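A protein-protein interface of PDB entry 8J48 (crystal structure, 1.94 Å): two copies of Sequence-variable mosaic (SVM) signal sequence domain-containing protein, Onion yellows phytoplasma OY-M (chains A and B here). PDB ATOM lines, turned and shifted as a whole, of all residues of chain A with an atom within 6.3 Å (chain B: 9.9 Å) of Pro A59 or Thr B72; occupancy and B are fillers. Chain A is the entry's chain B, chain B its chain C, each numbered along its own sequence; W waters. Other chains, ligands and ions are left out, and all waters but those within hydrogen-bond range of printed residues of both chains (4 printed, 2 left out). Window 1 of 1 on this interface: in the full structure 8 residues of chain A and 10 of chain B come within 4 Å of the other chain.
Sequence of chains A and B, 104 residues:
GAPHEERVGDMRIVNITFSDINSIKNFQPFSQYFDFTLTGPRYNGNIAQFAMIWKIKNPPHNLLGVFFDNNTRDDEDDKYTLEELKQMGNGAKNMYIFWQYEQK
OD1 of Asn B71 lies within hydrogen-bond range of NZ of Lys A55, 2.8 Å away. The backbone carbonyl oxygen (O) of Gly B91 lies within hydrogen-bond range of the side-chain amino group (NZ) of Lys A55 (3.1 Å). The backbone NH (N) of Asn A58 lies within hydrogen-bond range of the side-chain amide oxygen (OD1) of Asn B70, 3.5 Å away. A ring nitrogen (NE2) of His A61 is in hydrogen-bond range of the backbone carbonyl oxygen of Gly B45, 3.2 Å away. A ring nitrogen (NE2) of His A61 lies within hydrogen-bond range of the backbone carbonyl oxygen (O) of Arg B73 (2.8 Å).
The side-chain amide nitrogen (ND2) of Asn B44 lies within hydrogen-bond range of the backbone carbonyl oxygen (O) of Asn B46 (3.1 Å). NH1 of Arg B73 sits at hydrogen-bond distance from O of Asn B44 (3.1 Å). The backbone carbonyl oxygen (O) of Gly B45 lies within hydrogen-bond range of the backbone NH (N) of Arg B73. OD1 of Asn B71 is in hydrogen-bond range of ND2 of Asn B70. The backbone carbonyl oxygen (O) of Thr B72 lies within hydrogen-bond range of the side-chain amide nitrogen (ND2) of Asn B90 (2.8 Å). The guanidinium group (NH2) of Arg B73 sits at hydrogen-bond distance from the backbone carbonyl oxygen (O) of Gly B89, 2.9 Å away.
ND2 of Asn B71 touches CA of Gly A40, 3.5 Å away. Lys A55 touches Asn B70 (CE to ND2, 3.5 Å). CG of Asn A58 touches CG2 of Ile B47, at 3.3 Å. OD1 of Asn B70 touches CD of Pro A59 (3.9 Å). Pro A59 touches Thr B72. C of Pro A60 touches CG2 of Thr B72 (3.7 Å). CB of Asn B46 touches CE1 of His A61 (3.7 Å). N of His A61 touches CG2 of Thr B72 (3.5 Å). Asp B75 touches His A61 (OD2 to CE1, 3.3 Å).
Of the printed residues of chain B, His A61 touches Gly B45 (3.2 Å), Asn B46 (3.7 Å), Thr B72 (3.5 Å), Arg B73 (2.8 Å) and Asp B75 (3.3 Å). Printed residues of chain A within 4 Å of Gly B45: His A61. Printed residues of chain A within 4 Å of Ile B47: Asn A58. Of chain A, only Pro A59, Pro A60 and His A61 come within 4 Å of Thr B72. Printed residues of chain A within 4 Å of Arg B73: His A61 (2.8 Å). The nearest residue of chain B that does not touch Pro A59 is Asn B71 (4.1 Å). The nearest residue of chain A that does not touch Thr B72 is Asn A62 (4.8 Å).
Of the 25 printed residues of chain B, 9 touch a printed residue of chain A. Hydrophobic or aromatic side chains of chain B that line the printed part of chain A: Ile B47. Of the 12 printed residues of chain A, 6 touch a printed residue of chain B. Hydrophobic or aromatic side chains of chain A within 4 Å of the printed part of chain B: Pro A59 and His A61. Among the printed residues, 14 pairs touch across the chains. Among the printed residues, no Asp or Glu carboxylate lies within 4 Å of a Lys or Arg side-chain nitrogen of the other chain.
No position is printed for both chains.
Water W4 lies within hydrogen-bond range of the backbone carbonyl oxygen of Pro A59 (2.8 Å), the backbone NH of Ile B47 (2.8 Å) and the backbone carbonyl oxygen of Asn B71 (3.0 Å). Water W1 lies within hydrogen-bond range of the backbone carbonyl oxygen of Ile B47 (2.8 Å), the side-chain amide nitrogen of Asn B46 (3.0 Å) and the backbone carbonyl oxygen of Pro A59 (3.2 Å). Water W2 lies within hydrogen-bond range of the backbone NH (N) of Asn A62 (2.8 Å) and the side-chain hydroxyl (OG1) of Thr B72 (3.1 Å). Water W3 lies within hydrogen-bond range of OG1 of Thr B72 and O of Pro A60.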
ATOM      1  N   GLY A  40     -21.555  35.108  23.465  1.00  0.00           N
ATOM      2  CA  GLY A  40     -22.429  34.103  24.025  1.00  0.00           C
ATOM      3  C   GLY A  40     -23.122  34.639  25.258  1.00  0.00           C
ATOM      4  O   GLY A  40     -22.558  35.445  26.008  1.00  0.00           O
ATOM      5  N   PRO A  41     -24.369  34.213  25.478  1.00  0.00           N
ATOM      6  CA  PRO A  41     -25.147  34.737  26.612  1.00  0.00           C
ATOM      7  C   PRO A  41     -24.604  34.288  27.965  1.00  0.00           C
ATOM      8  O   PRO A  41     -24.176  33.142  28.147  1.00  0.00           O
ATOM      9  CB  PRO A  41     -26.557  34.174  26.373  1.00  0.00           C
ATOM     10  CG  PRO A  41     -26.341  32.942  25.517  1.00  0.00           C
ATOM     11  CD  PRO A  41     -25.155  33.305  24.624  1.00  0.00           C
ATOM     12  N   LYS A  55     -20.839  31.791  31.555  1.00  0.00           N
ATOM     13  CA  LYS A  55     -21.325  31.364  30.246  1.00  0.00           C
ATOM     14  C   LYS A  55     -22.399  30.288  30.385  1.00  0.00           C
ATOM     15  O   LYS A  55     -22.148  29.210  30.935  1.00  0.00           O
ATOM     16  CB  LYS A  55     -20.182  30.863  29.367  1.00  0.00           C
ATOM     17  CG  LYS A  55     -20.345  31.304  27.916  1.00  0.00           C
ATOM     18  CD  LYS A  55     -19.619  30.369  26.945  1.00  0.00           C
ATOM     19  CE  LYS A  55     -20.119  30.569  25.511  1.00  0.00           C
ATOM     20  NZ  LYS A  55     -19.009  30.424  24.510  1.00  0.00           N
ATOM     21  N   ILE A  56     -23.585  30.583  29.845  1.00  0.00           N
ATOM     22  CA  ILE A  56     -24.684  29.633  29.807  1.00  0.00           C
ATOM     23  C   ILE A  56     -24.360  28.496  28.849  1.00  0.00           C
ATOM     24  O   ILE A  56     -23.888  28.719  27.732  1.00  0.00           O
ATOM     25  CB  ILE A  56     -25.970  30.352  29.379  1.00  0.00           C
ATOM     26  CG1 ILE A  56     -26.312  31.419  30.422  1.00  0.00           C
ATOM     27  CG2 ILE A  56     -27.095  29.330  29.128  1.00  0.00           C
ATOM     28  CD1 ILE A  56     -27.465  32.329  30.037  1.00  0.00           C
ATOM     29  N   LYS A  57     -24.635  27.271  29.279  1.00  0.00           N
ATOM     30  CA  LYS A  57     -24.301  26.094  28.494  1.00  0.00           C
ATOM     31  C   LYS A  57     -25.382  25.785  27.462  1.00  0.00           C
ATOM     32  O   LYS A  57     -26.578  25.870  27.752  1.00  0.00           O
ATOM     33  CB  LYS A  57     -24.107  24.884  29.410  1.00  0.00           C
ATOM     34  CG  LYS A  57     -23.819  23.594  28.637  1.00  0.00           C
ATOM     35  CD  LYS A  57     -23.317  22.494  29.548  1.00  0.00           C
ATOM     36  CE  LYS A  57     -24.452  21.656  30.071  1.00  0.00           C
ATOM     37  NZ  LYS A  57     -23.909  20.449  30.777  1.00  0.00           N
ATOM     38  N   ASN A  58     -24.942  25.411  26.253  1.00  0.00           N
ATOM     39  CA  ASN A  58     -25.813  24.948  25.184  1.00  0.00           C
ATOM     40  C   ASN A  58     -27.009  25.883  24.952  1.00  0.00           C
ATOM     41  O   ASN A  58     -28.146  25.444  24.937  1.00  0.00           O
ATOM     42  CB  ASN A  58     -26.314  23.536  25.469  1.00  0.00           C
ATOM     43  CG  ASN A  58     -25.183  22.544  25.637  1.00  0.00           C
ATOM     44  OD1 ASN A  58     -24.030  22.835  25.318  1.00  0.00           O
ATOM     45  ND2 ASN A  58     -25.518  21.351  26.106  1.00  0.00           N
ATOM     46  N   PRO A  59     -26.754  27.185  24.774  1.00  0.00           N
ATOM     47  CA  PRO A  59     -27.870  28.129  24.760  1.00  0.00           C
ATOM     48  C   PRO A  59     -28.728  27.931  23.499  1.00  0.00           C
ATOM     49  O   PRO A  59     -28.228  27.445  22.483  1.00  0.00           O
ATOM     50  CB  PRO A  59     -27.174  29.499  24.746  1.00  0.00           C
ATOM     51  CG  PRO A  59     -25.891  29.240  24.038  1.00  0.00           C
ATOM     52  CD  PRO A  59     -25.471  27.862  24.493  1.00  0.00           C
ATOM     53  N   PRO A  60     -30.006  28.261  23.585  1.00  0.00           N
ATOM     54  CA  PRO A  60     -30.817  28.316  22.361  1.00  0.00           C
ATOM     55  C   PRO A  60     -30.511  29.575  21.566  1.00  0.00           C
ATOM     56  O   PRO A  60     -29.967  30.551  22.083  1.00  0.00           O
ATOM     57  CB  PRO A  60     -32.249  28.339  22.905  1.00  0.00           C
ATOM     58  CG  PRO A  60     -32.104  29.150  24.224  1.00  0.00           C
ATOM     59  CD  PRO A  60     -30.766  28.648  24.787  1.00  0.00           C
ATOM     60  N   HIS A  61     -30.891  29.544  20.285  1.00  0.00           N
ATOM     61  CA  HIS A  61     -30.790  30.723  19.424  1.00  0.00           C
ATOM     62  C   HIS A  61     -31.465  31.926  20.061  1.00  0.00           C
ATOM     63  O   HIS A  61     -32.525  31.796  20.676  1.00  0.00           O
ATOM     64  CB  HIS A  61     -31.463  30.460  18.066  1.00  0.00           C
ATOM     65  CG  HIS A  61     -30.663  29.590  17.145  1.00  0.00           C
ATOM     66  ND1 HIS A  61     -30.753  28.214  17.157  1.00  0.00           N
ATOM     67  CD2 HIS A  61     -29.762  29.902  16.183  1.00  0.00           C
ATOM     68  CE1 HIS A  61     -29.942  27.716  16.244  1.00  0.00           C
ATOM     69  NE2 HIS A  61     -29.322  28.719  15.644  1.00  0.00           N
ATOM     70  N   ASN A  62     -30.855  33.100  19.883  1.00  0.00           N
ATOM     71  CA  ASN A  62     -31.388  34.427  20.179  1.00  0.00           C
ATOM     72  C   ASN A  62     -31.322  34.772  21.663  1.00  0.00           C
ATOM     73  O   ASN A  62     -31.693  35.897  22.036  1.00  0.00           O
ATOM     74  CB  ASN A  62     -32.835  34.598  19.687  1.00  0.00           C
ATOM     75  CG  ASN A  62     -32.961  34.343  18.197  1.00  0.00           C
ATOM     76  OD1 ASN A  62     -32.186  34.882  17.419  1.00  0.00           O
ATOM     77  ND2 ASN A  62     -33.907  33.495  17.798  1.00  0.00           N
ATOM     78  N   LEU A  63     -30.848  33.868  22.516  1.00  0.00           N
ATOM     79  CA  LEU A  63     -30.654  34.202  23.920  1.00  0.00           C
ATOM     80  C   LEU A  63     -29.477  35.156  24.063  1.00  0.00           C
ATOM     81  O   LEU A  63     -28.385  34.898  23.552  1.00  0.00           O
ATOM     82  CB  LEU A  63     -30.432  32.942  24.747  1.00  0.00           C
ATOM     83  CG  LEU A  63     -30.147  33.194  26.231  1.00  0.00           C
ATOM     84  CD1 LEU A  63     -31.358  33.850  26.919  1.00  0.00           C
ATOM     85  CD2 LEU A  63     -29.701  31.917  26.995  1.00  0.00           C
ATOM     86  N   LEU A  82     -30.054  27.023  30.263  1.00  0.00           N
ATOM     87  CA  LEU A  82     -31.118  27.947  30.637  1.00  0.00           C
ATOM     88  C   LEU A  82     -32.171  27.274  31.515  1.00  0.00           C
ATOM     89  O   LEU A  82     -32.659  27.875  32.481  1.00  0.00           O
ATOM     90  CB  LEU A  82     -31.777  28.505  29.371  1.00  0.00           C
ATOM     91  CG  LEU A  82     -32.831  29.575  29.635  1.00  0.00           C
ATOM     92  CD1 LEU A  82     -32.139  30.751  30.345  1.00  0.00           C
ATOM     93  CD2 LEU A  82     -33.545  30.011  28.343  1.00  0.00           C
ATOM     94  N   MET B  11     -11.534  29.714  18.564  1.00  0.00           N
ATOM     95  CA  MET B  11     -12.050  28.403  18.207  1.00  0.00           C
ATOM     96  C   MET B  11     -10.971  27.597  17.493  1.00  0.00           C
ATOM     97  O   MET B  11     -10.360  28.074  16.531  1.00  0.00           O
ATOM     98  CB  MET B  11     -13.281  28.530  17.317  1.00  0.00           C
ATOM     99  CG  MET B  11     -13.930  27.206  17.019  1.00  0.00           C
ATOM    100  SD  MET B  11     -15.388  27.469  16.004  1.00  0.00           S
ATOM    101  CE  MET B  11     -14.662  27.950  14.435  1.00  0.00           C
ATOM    102  N   TYR B  43     -24.069  20.076   9.397  1.00  0.00           N
ATOM    103  CA  TYR B  43     -23.534  20.805  10.543  1.00  0.00           C
ATOM    104  C   TYR B  43     -24.674  21.132  11.503  1.00  0.00           C
ATOM    105  O   TYR B  43     -25.848  21.079  11.137  1.00  0.00           O
ATOM    106  CB  TYR B  43     -22.806  22.080  10.104  1.00  0.00           C
ATOM    107  CG  TYR B  43     -23.706  23.251   9.725  1.00  0.00           C
ATOM    108  CD1 TYR B  43     -24.209  23.392   8.436  1.00  0.00           C
ATOM    109  CD2 TYR B  43     -24.042  24.224  10.663  1.00  0.00           C
ATOM    110  CE1 TYR B  43     -25.042  24.484   8.087  1.00  0.00           C
ATOM    111  CE2 TYR B  43     -24.886  25.304  10.326  1.00  0.00           C
ATOM    112  CZ  TYR B  43     -25.371  25.430   9.039  1.00  0.00           C
ATOM    113  OH  TYR B  43     -26.164  26.519   8.732  1.00  0.00           O
ATOM    114  N   ASN B  44     -24.326  21.462  12.747  1.00  0.00           N
ATOM    115  CA  ASN B  44     -25.316  21.851  13.749  1.00  0.00           C
ATOM    116  C   ASN B  44     -25.326  23.360  13.935  1.00  0.00           C
ATOM    117  O   ASN B  44     -24.277  24.006  13.947  1.00  0.00           O
ATOM    118  CB  ASN B  44     -25.053  21.191  15.106  1.00  0.00           C
ATOM    119  CG  ASN B  44     -23.706  21.525  15.649  1.00  0.00           C
ATOM    120  OD1 ASN B  44     -22.706  21.441  14.932  1.00  0.00           O
ATOM    121  ND2 ASN B  44     -23.655  21.909  16.928  1.00  0.00           N
ATOM    122  N   GLY B  45     -26.522  23.911  14.097  1.00  0.00           N
ATOM    123  CA  GLY B  45     -26.662  25.323  14.373  1.00  0.00           C
ATOM    124  C   GLY B  45     -26.758  25.651  15.836  1.00  0.00           C
ATOM    125  O   GLY B  45     -26.819  26.828  16.196  1.00  0.00           O
ATOM    126  N   ASN B  46     -26.732  24.633  16.695  1.00  0.00           N
ATOM    127  CA  ASN B  46     -26.935  24.775  18.128  1.00  0.00           C
ATOM    128  C   ASN B  46     -26.641  23.421  18.749  1.00  0.00           C
ATOM    129  O   ASN B  46     -26.453  22.427  18.044  1.00  0.00           O
ATOM    130  CB  ASN B  46     -28.360  25.218  18.443  1.00  0.00           C
ATOM    131  CG  ASN B  46     -29.390  24.263  17.881  1.00  0.00           C
ATOM    132  OD1 ASN B  46     -29.504  24.076  16.655  1.00  0.00           O
ATOM    133  ND2 ASN B  46     -30.135  23.637  18.768  1.00  0.00           N
ATOM    134  N   ILE B  47     -26.603  23.379  20.077  1.00  0.00           N
ATOM    135  CA  ILE B  47     -26.395  22.114  20.768  1.00  0.00           C
ATOM    136  C   ILE B  47     -27.747  21.514  21.108  1.00  0.00           C
ATOM    137  O   ILE B  47     -28.522  22.097  21.876  1.00  0.00           O
ATOM    138  CB  ILE B  47     -25.524  22.277  22.020  1.00  0.00           C
ATOM    139  CG1 ILE B  47     -24.128  22.728  21.607  1.00  0.00           C
ATOM    140  CG2 ILE B  47     -25.442  20.937  22.776  1.00  0.00           C
ATOM    141  CD1 ILE B  47     -23.413  21.691  20.733  1.00  0.00           C
ATOM    142  N   ALA B  48     -28.033  20.358  20.517  1.00  0.00           N
ATOM    143  CA  ALA B  48     -29.233  19.588  20.805  1.00  0.00           C
ATOM    144  C   ALA B  48     -28.934  18.140  20.456  1.00  0.00           C
ATOM    145  O   ALA B  48     -27.902  17.835  19.860  1.00  0.00           O
ATOM    146  CB  ALA B  48     -30.440  20.111  20.015  1.00  0.00           C
ATOM    147  N   ALA B  51     -28.131  17.068  16.518  1.00  0.00           N
ATOM    148  CA  ALA B  51     -28.409  18.366  15.916  1.00  0.00           C
ATOM    149  C   ALA B  51     -27.703  18.603  14.580  1.00  0.00           C
ATOM    150  O   ALA B  51     -27.968  19.622  13.930  1.00  0.00           O
ATOM    151  CB  ALA B  51     -28.006  19.472  16.893  1.00  0.00           C
ATOM    152  N   TRP B  54     -28.235  20.244   9.266  1.00  0.00           N
ATOM    153  CA  TRP B  54     -28.264  21.250   8.204  1.00  0.00           C
ATOM    154  C   TRP B  54     -27.245  20.950   7.108  1.00  0.00           C
ATOM    155  O   TRP B  54     -26.052  20.780   7.388  1.00  0.00           O
ATOM    156  CB  TRP B  54     -28.016  22.628   8.805  1.00  0.00           C
ATOM    157  CG  TRP B  54     -29.050  22.923   9.846  1.00  0.00           C
ATOM    158  CD1 TRP B  54     -28.906  22.858  11.216  1.00  0.00           C
ATOM    159  CD2 TRP B  54     -30.411  23.285   9.600  1.00  0.00           C
ATOM    160  NE1 TRP B  54     -30.104  23.185  11.829  1.00  0.00           N
ATOM    161  CE2 TRP B  54     -31.042  23.442  10.858  1.00  0.00           C
ATOM    162  CE3 TRP B  54     -31.159  23.509   8.433  1.00  0.00           C
ATOM    163  CZ2 TRP B  54     -32.388  23.833  10.977  1.00  0.00           C
ATOM    164  CZ3 TRP B  54     -32.505  23.882   8.554  1.00  0.00           C
ATOM    165  CH2 TRP B  54     -33.098  24.040   9.821  1.00  0.00           C
ATOM    166  N   PHE B  68     -20.005  21.932  15.806  1.00  0.00           N
ATOM    167  CA  PHE B  68     -19.606  23.062  16.646  1.00  0.00           C
ATOM    168  C   PHE B  68     -19.941  22.745  18.102  1.00  0.00           C
ATOM    169  O   PHE B  68     -21.089  22.419  18.410  1.00  0.00           O
ATOM    170  CB  PHE B  68     -20.345  24.340  16.233  1.00  0.00           C
ATOM    171  CG  PHE B  68     -19.973  24.877  14.870  1.00  0.00           C
ATOM    172  CD1 PHE B  68     -20.723  24.542  13.753  1.00  0.00           C
ATOM    173  CD2 PHE B  68     -18.890  25.733  14.719  1.00  0.00           C
ATOM    174  CE1 PHE B  68     -20.401  25.041  12.485  1.00  0.00           C
ATOM    175  CE2 PHE B  68     -18.548  26.240  13.465  1.00  0.00           C
ATOM    176  CZ  PHE B  68     -19.308  25.892  12.344  1.00  0.00           C
ATOM    177  N   ASP B  69     -18.927  22.747  18.972  1.00  0.00           N
ATOM    178  CA  ASP B  69     -19.111  22.257  20.369  1.00  0.00           C
ATOM    179  C   ASP B  69     -19.996  23.143  21.250  1.00  0.00           C
ATOM    180  O   ASP B  69     -20.336  22.681  22.352  1.00  0.00           O
ATOM    181  CB  ASP B  69     -17.769  21.911  21.022  1.00  0.00           C
ATOM    182  CG  ASP B  69     -16.941  23.101  21.466  1.00  0.00           C
ATOM    183  OD1 ASP B  69     -17.170  24.205  20.952  1.00  0.00           O
ATOM    184  OD2 ASP B  69     -16.053  22.904  22.314  1.00  0.00           O
ATOM    185  N   ASN B  70     -20.355  24.344  20.799  1.00  0.00           N
ATOM    186  CA  ASN B  70     -21.123  25.227  21.709  1.00  0.00           C
ATOM    187  C   ASN B  70     -21.742  26.398  20.953  1.00  0.00           C
ATOM    188  O   ASN B  70     -21.370  26.589  19.782  1.00  0.00           O
ATOM    189  CB  ASN B  70     -20.229  25.775  22.824  1.00  0.00           C
ATOM    190  CG  ASN B  70     -20.999  26.275  24.025  1.00  0.00           C
ATOM    191  OD1 ASN B  70     -22.115  25.830  24.288  1.00  0.00           O
ATOM    192  ND2 ASN B  70     -20.418  27.215  24.747  1.00  0.00           N
ATOM    193  N   ASN B  71     -22.682  27.100  21.590  1.00  0.00           N
ATOM    194  CA  ASN B  71     -23.274  28.337  21.018  1.00  0.00           C
ATOM    195  C   ASN B  71     -24.178  28.069  19.821  1.00  0.00           C
ATOM    196  O   ASN B  71     -24.528  26.905  19.573  1.00  0.00           O
ATOM    197  CB  ASN B  71     -22.233  29.426  20.776  1.00  0.00           C
ATOM    198  CG  ASN B  71     -21.613  29.880  22.075  1.00  0.00           C
ATOM    199  OD1 ASN B  71     -20.631  29.301  22.523  1.00  0.00           O
ATOM    200  ND2 ASN B  71     -22.202  30.884  22.701  1.00  0.00           N
ATOM    201  N   THR B  72     -24.556  29.141  19.128  1.00  0.00           N
ATOM    202  CA  THR B  72     -25.533  28.989  18.030  1.00  0.00           C
ATOM    203  C   THR B  72     -25.051  29.706  16.774  1.00  0.00           C
ATOM    204  O   THR B  72     -24.139  30.533  16.893  1.00  0.00           O
ATOM    205  CB  THR B  72     -26.894  29.564  18.434  1.00  0.00           C
ATOM    206  OG1 THR B  72     -26.703  30.924  18.824  1.00  0.00           O
ATOM    207  CG2 THR B  72     -27.551  28.787  19.552  1.00  0.00           C
ATOM    208  N   ARG B  73     -25.658  29.392  15.629  1.00  0.00           N
ATOM    209  CA  ARG B  73     -25.327  30.060  14.378  1.00  0.00           C
ATOM    210  C   ARG B  73     -26.495  29.883  13.414  1.00  0.00           C
ATOM    211  O   ARG B  73     -27.370  29.031  13.613  1.00  0.00           O
ATOM    212  CB  ARG B  73     -24.010  29.518  13.792  1.00  0.00           C
ATOM    213  CG  ARG B  73     -24.058  28.049  13.393  1.00  0.00           C
ATOM    214  CD  ARG B  73     -22.684  27.371  13.489  1.00  0.00           C
ATOM    215  NE  ARG B  73     -22.028  27.653  14.759  1.00  0.00           N
ATOM    216  CZ  ARG B  73     -22.289  27.022  15.905  1.00  0.00           C
ATOM    217  NH1 ARG B  73     -23.192  26.042  15.965  1.00  0.00           N
ATOM    218  NH2 ARG B  73     -21.639  27.380  16.994  1.00  0.00           N
ATOM    219  N   ASP B  74     -26.500  30.692  12.360  1.00  0.00           N
ATOM    220  CA  ASP B  74     -27.565  30.584  11.363  1.00  0.00           C
ATOM    221  C   ASP B  74     -27.614  29.155  10.825  1.00  0.00           C
ATOM    222  O   ASP B  74     -26.583  28.557  10.492  1.00  0.00           O
ATOM    223  CB  ASP B  74     -27.361  31.589  10.219  1.00  0.00           C
ATOM    224  CG  ASP B  74     -28.573  31.646   9.252  1.00  0.00           C
ATOM    225  OD1 ASP B  74     -29.722  31.632   9.737  1.00  0.00           O
ATOM    226  OD2 ASP B  74     -28.385  31.713   8.007  1.00  0.00           O
ATOM    227  N   ASP B  75     -28.817  28.599  10.790  1.00  0.00           N
ATOM    228  CA  ASP B  75     -29.047  27.186  10.535  1.00  0.00           C
ATOM    229  C   ASP B  75     -29.933  27.106   9.294  1.00  0.00           C
ATOM    230  O   ASP B  75     -31.137  27.350   9.375  1.00  0.00           O
ATOM    231  CB  ASP B  75     -29.688  26.491  11.745  1.00  0.00           C
ATOM    232  CG  ASP B  75     -30.792  27.322  12.421  1.00  0.00           C
ATOM    233  OD1 ASP B  75     -31.072  28.477  12.007  1.00  0.00           O
ATOM    234  OD2 ASP B  75     -31.393  26.797  13.383  1.00  0.00           O
ATOM    235  N   LEU B  85     -18.482  28.233   7.177  1.00  0.00           N
ATOM    236  CA  LEU B  85     -18.778  27.708   8.499  1.00  0.00           C
ATOM    237  C   LEU B  85     -17.607  27.889   9.462  1.00  0.00           C
ATOM    238  O   LEU B  85     -17.826  28.063  10.667  1.00  0.00           O
ATOM    239  CB  LEU B  85     -19.189  26.239   8.378  1.00  0.00           C
ATOM    240  CG  LEU B  85     -20.618  26.019   7.853  1.00  0.00           C
ATOM    241  CD1 LEU B  85     -20.885  24.557   7.518  1.00  0.00           C
ATOM    242  CD2 LEU B  85     -21.644  26.518   8.875  1.00  0.00           C
ATOM    243  N   GLN B  87     -15.992  30.455   9.902  1.00  0.00           N
ATOM    244  CA  GLN B  87     -16.100  31.790  10.464  1.00  0.00           C
ATOM    245  C   GLN B  87     -17.345  31.951  11.315  1.00  0.00           C
ATOM    246  O   GLN B  87     -17.633  33.058  11.780  1.00  0.00           O
ATOM    247  CB  GLN B  87     -16.085  32.829   9.344  1.00  0.00           C
ATOM    248  CG  GLN B  87     -14.823  32.777   8.493  1.00  0.00           C
ATOM    249  CD  GLN B  87     -13.551  33.008   9.305  1.00  0.00           C
ATOM    250  OE1 GLN B  87     -13.527  33.792  10.252  1.00  0.00           O
ATOM    251  NE2 GLN B  87     -12.496  32.315   8.932  1.00  0.00           N
ATOM    252  N   MET B  88     -18.095  30.878  11.527  1.00  0.00           N
ATOM    253  CA  MET B  88     -19.395  30.987  12.163  1.00  0.00           C
ATOM    254  C   MET B  88     -19.433  30.257  13.504  1.00  0.00           C
ATOM    255  O   MET B  88     -20.496  29.817  13.944  1.00  0.00           O
ATOM    256  CB  MET B  88     -20.484  30.485  11.216  1.00  0.00           C
ATOM    257  CG  MET B  88     -20.512  31.253   9.903  1.00  0.00           C
ATOM    258  SD  MET B  88     -21.542  30.482   8.638  1.00  0.00           S
ATOM    259  CE  MET B  88     -23.132  30.395   9.478  1.00  0.00           C
ATOM    260  N   GLY B  89     -18.277  30.166  14.183  1.00  0.00           N
ATOM    261  CA  GLY B  89     -18.242  29.540  15.498  1.00  0.00           C
ATOM    262  C   GLY B  89     -19.091  30.269  16.526  1.00  0.00           C
ATOM    263  O   GLY B  89     -19.788  29.640  17.323  1.00  0.00           O
ATOM    264  N   ASN B  90     -19.023  31.602  16.540  1.00  0.00           N
ATOM    265  CA  ASN B  90     -19.891  32.430  17.396  1.00  0.00           C
ATOM    266  C   ASN B  90     -19.792  32.020  18.872  1.00  0.00           C
ATOM    267  O   ASN B  90     -20.777  32.028  19.617  1.00  0.00           O
ATOM    268  CB  ASN B  90     -21.340  32.380  16.883  1.00  0.00           C
ATOM    269  CG  ASN B  90     -22.216  33.490  17.451  1.00  0.00           C
ATOM    270  OD1 ASN B  90     -21.738  34.596  17.726  1.00  0.00           O
ATOM    271  ND2 ASN B  90     -23.516  33.203  17.620  1.00  0.00           N
ATOM    272  N   GLY B  91     -18.587  31.658  19.312  1.00  0.00           N
ATOM    273  CA  GLY B  91     -18.336  31.316  20.697  1.00  0.00           C
ATOM    274  C   GLY B  91     -17.953  29.866  20.943  1.00  0.00           C
ATOM    275  O   GLY B  91     -17.429  29.554  22.029  1.00  0.00           O
ATOM    276  N   ALA B  92     -18.232  28.969  19.995  1.00  0.00           N
ATOM    277  CA  ALA B  92     -17.763  27.593  20.104  1.00  0.00           C
ATOM    278  C   ALA B  92     -16.259  27.559  20.350  1.00  0.00           C
ATOM    279  O   ALA B  92     -15.500  28.314  19.743  1.00  0.00           O
ATOM    280  CB  ALA B  92     -18.105  26.818  18.826  1.00  0.00           C
ATOM    281  N   LYS B  93     -15.818  26.684  21.242  1.00  0.00           N
ATOM    282  CA  LYS B  93     -14.376  26.584  21.451  1.00  0.00           C
ATOM    283  C   LYS B  93     -13.707  25.583  20.526  1.00  0.00           C
ATOM    284  O   LYS B  93     -12.486  25.645  20.361  1.00  0.00           O
ATOM    285  CB  LYS B  93     -14.057  26.236  22.912  1.00  0.00           C
ATOM    286  CG  LYS B  93     -14.662  27.240  23.882  1.00  0.00           C
ATOM    287  CD  LYS B  93     -13.783  28.475  24.041  1.00  0.00           C
ATOM    288  CE  LYS B  93     -14.484  29.554  24.878  1.00  0.00           C
ATOM    289  NZ  LYS B  93     -13.919  30.926  24.652  1.00  0.00           N
HETATM  290  O   HOH W   1     -29.501  24.719  21.529  1.00  0.00           O
HETATM  291  O   HOH W   2     -28.593  33.262  18.186  1.00  0.00           O
HETATM  292  O   HOH W   3     -27.379  31.854  21.532  1.00  0.00           O
HETATM  293  O   HOH W   4     -26.227  25.666  21.711  1.00  0.00           O
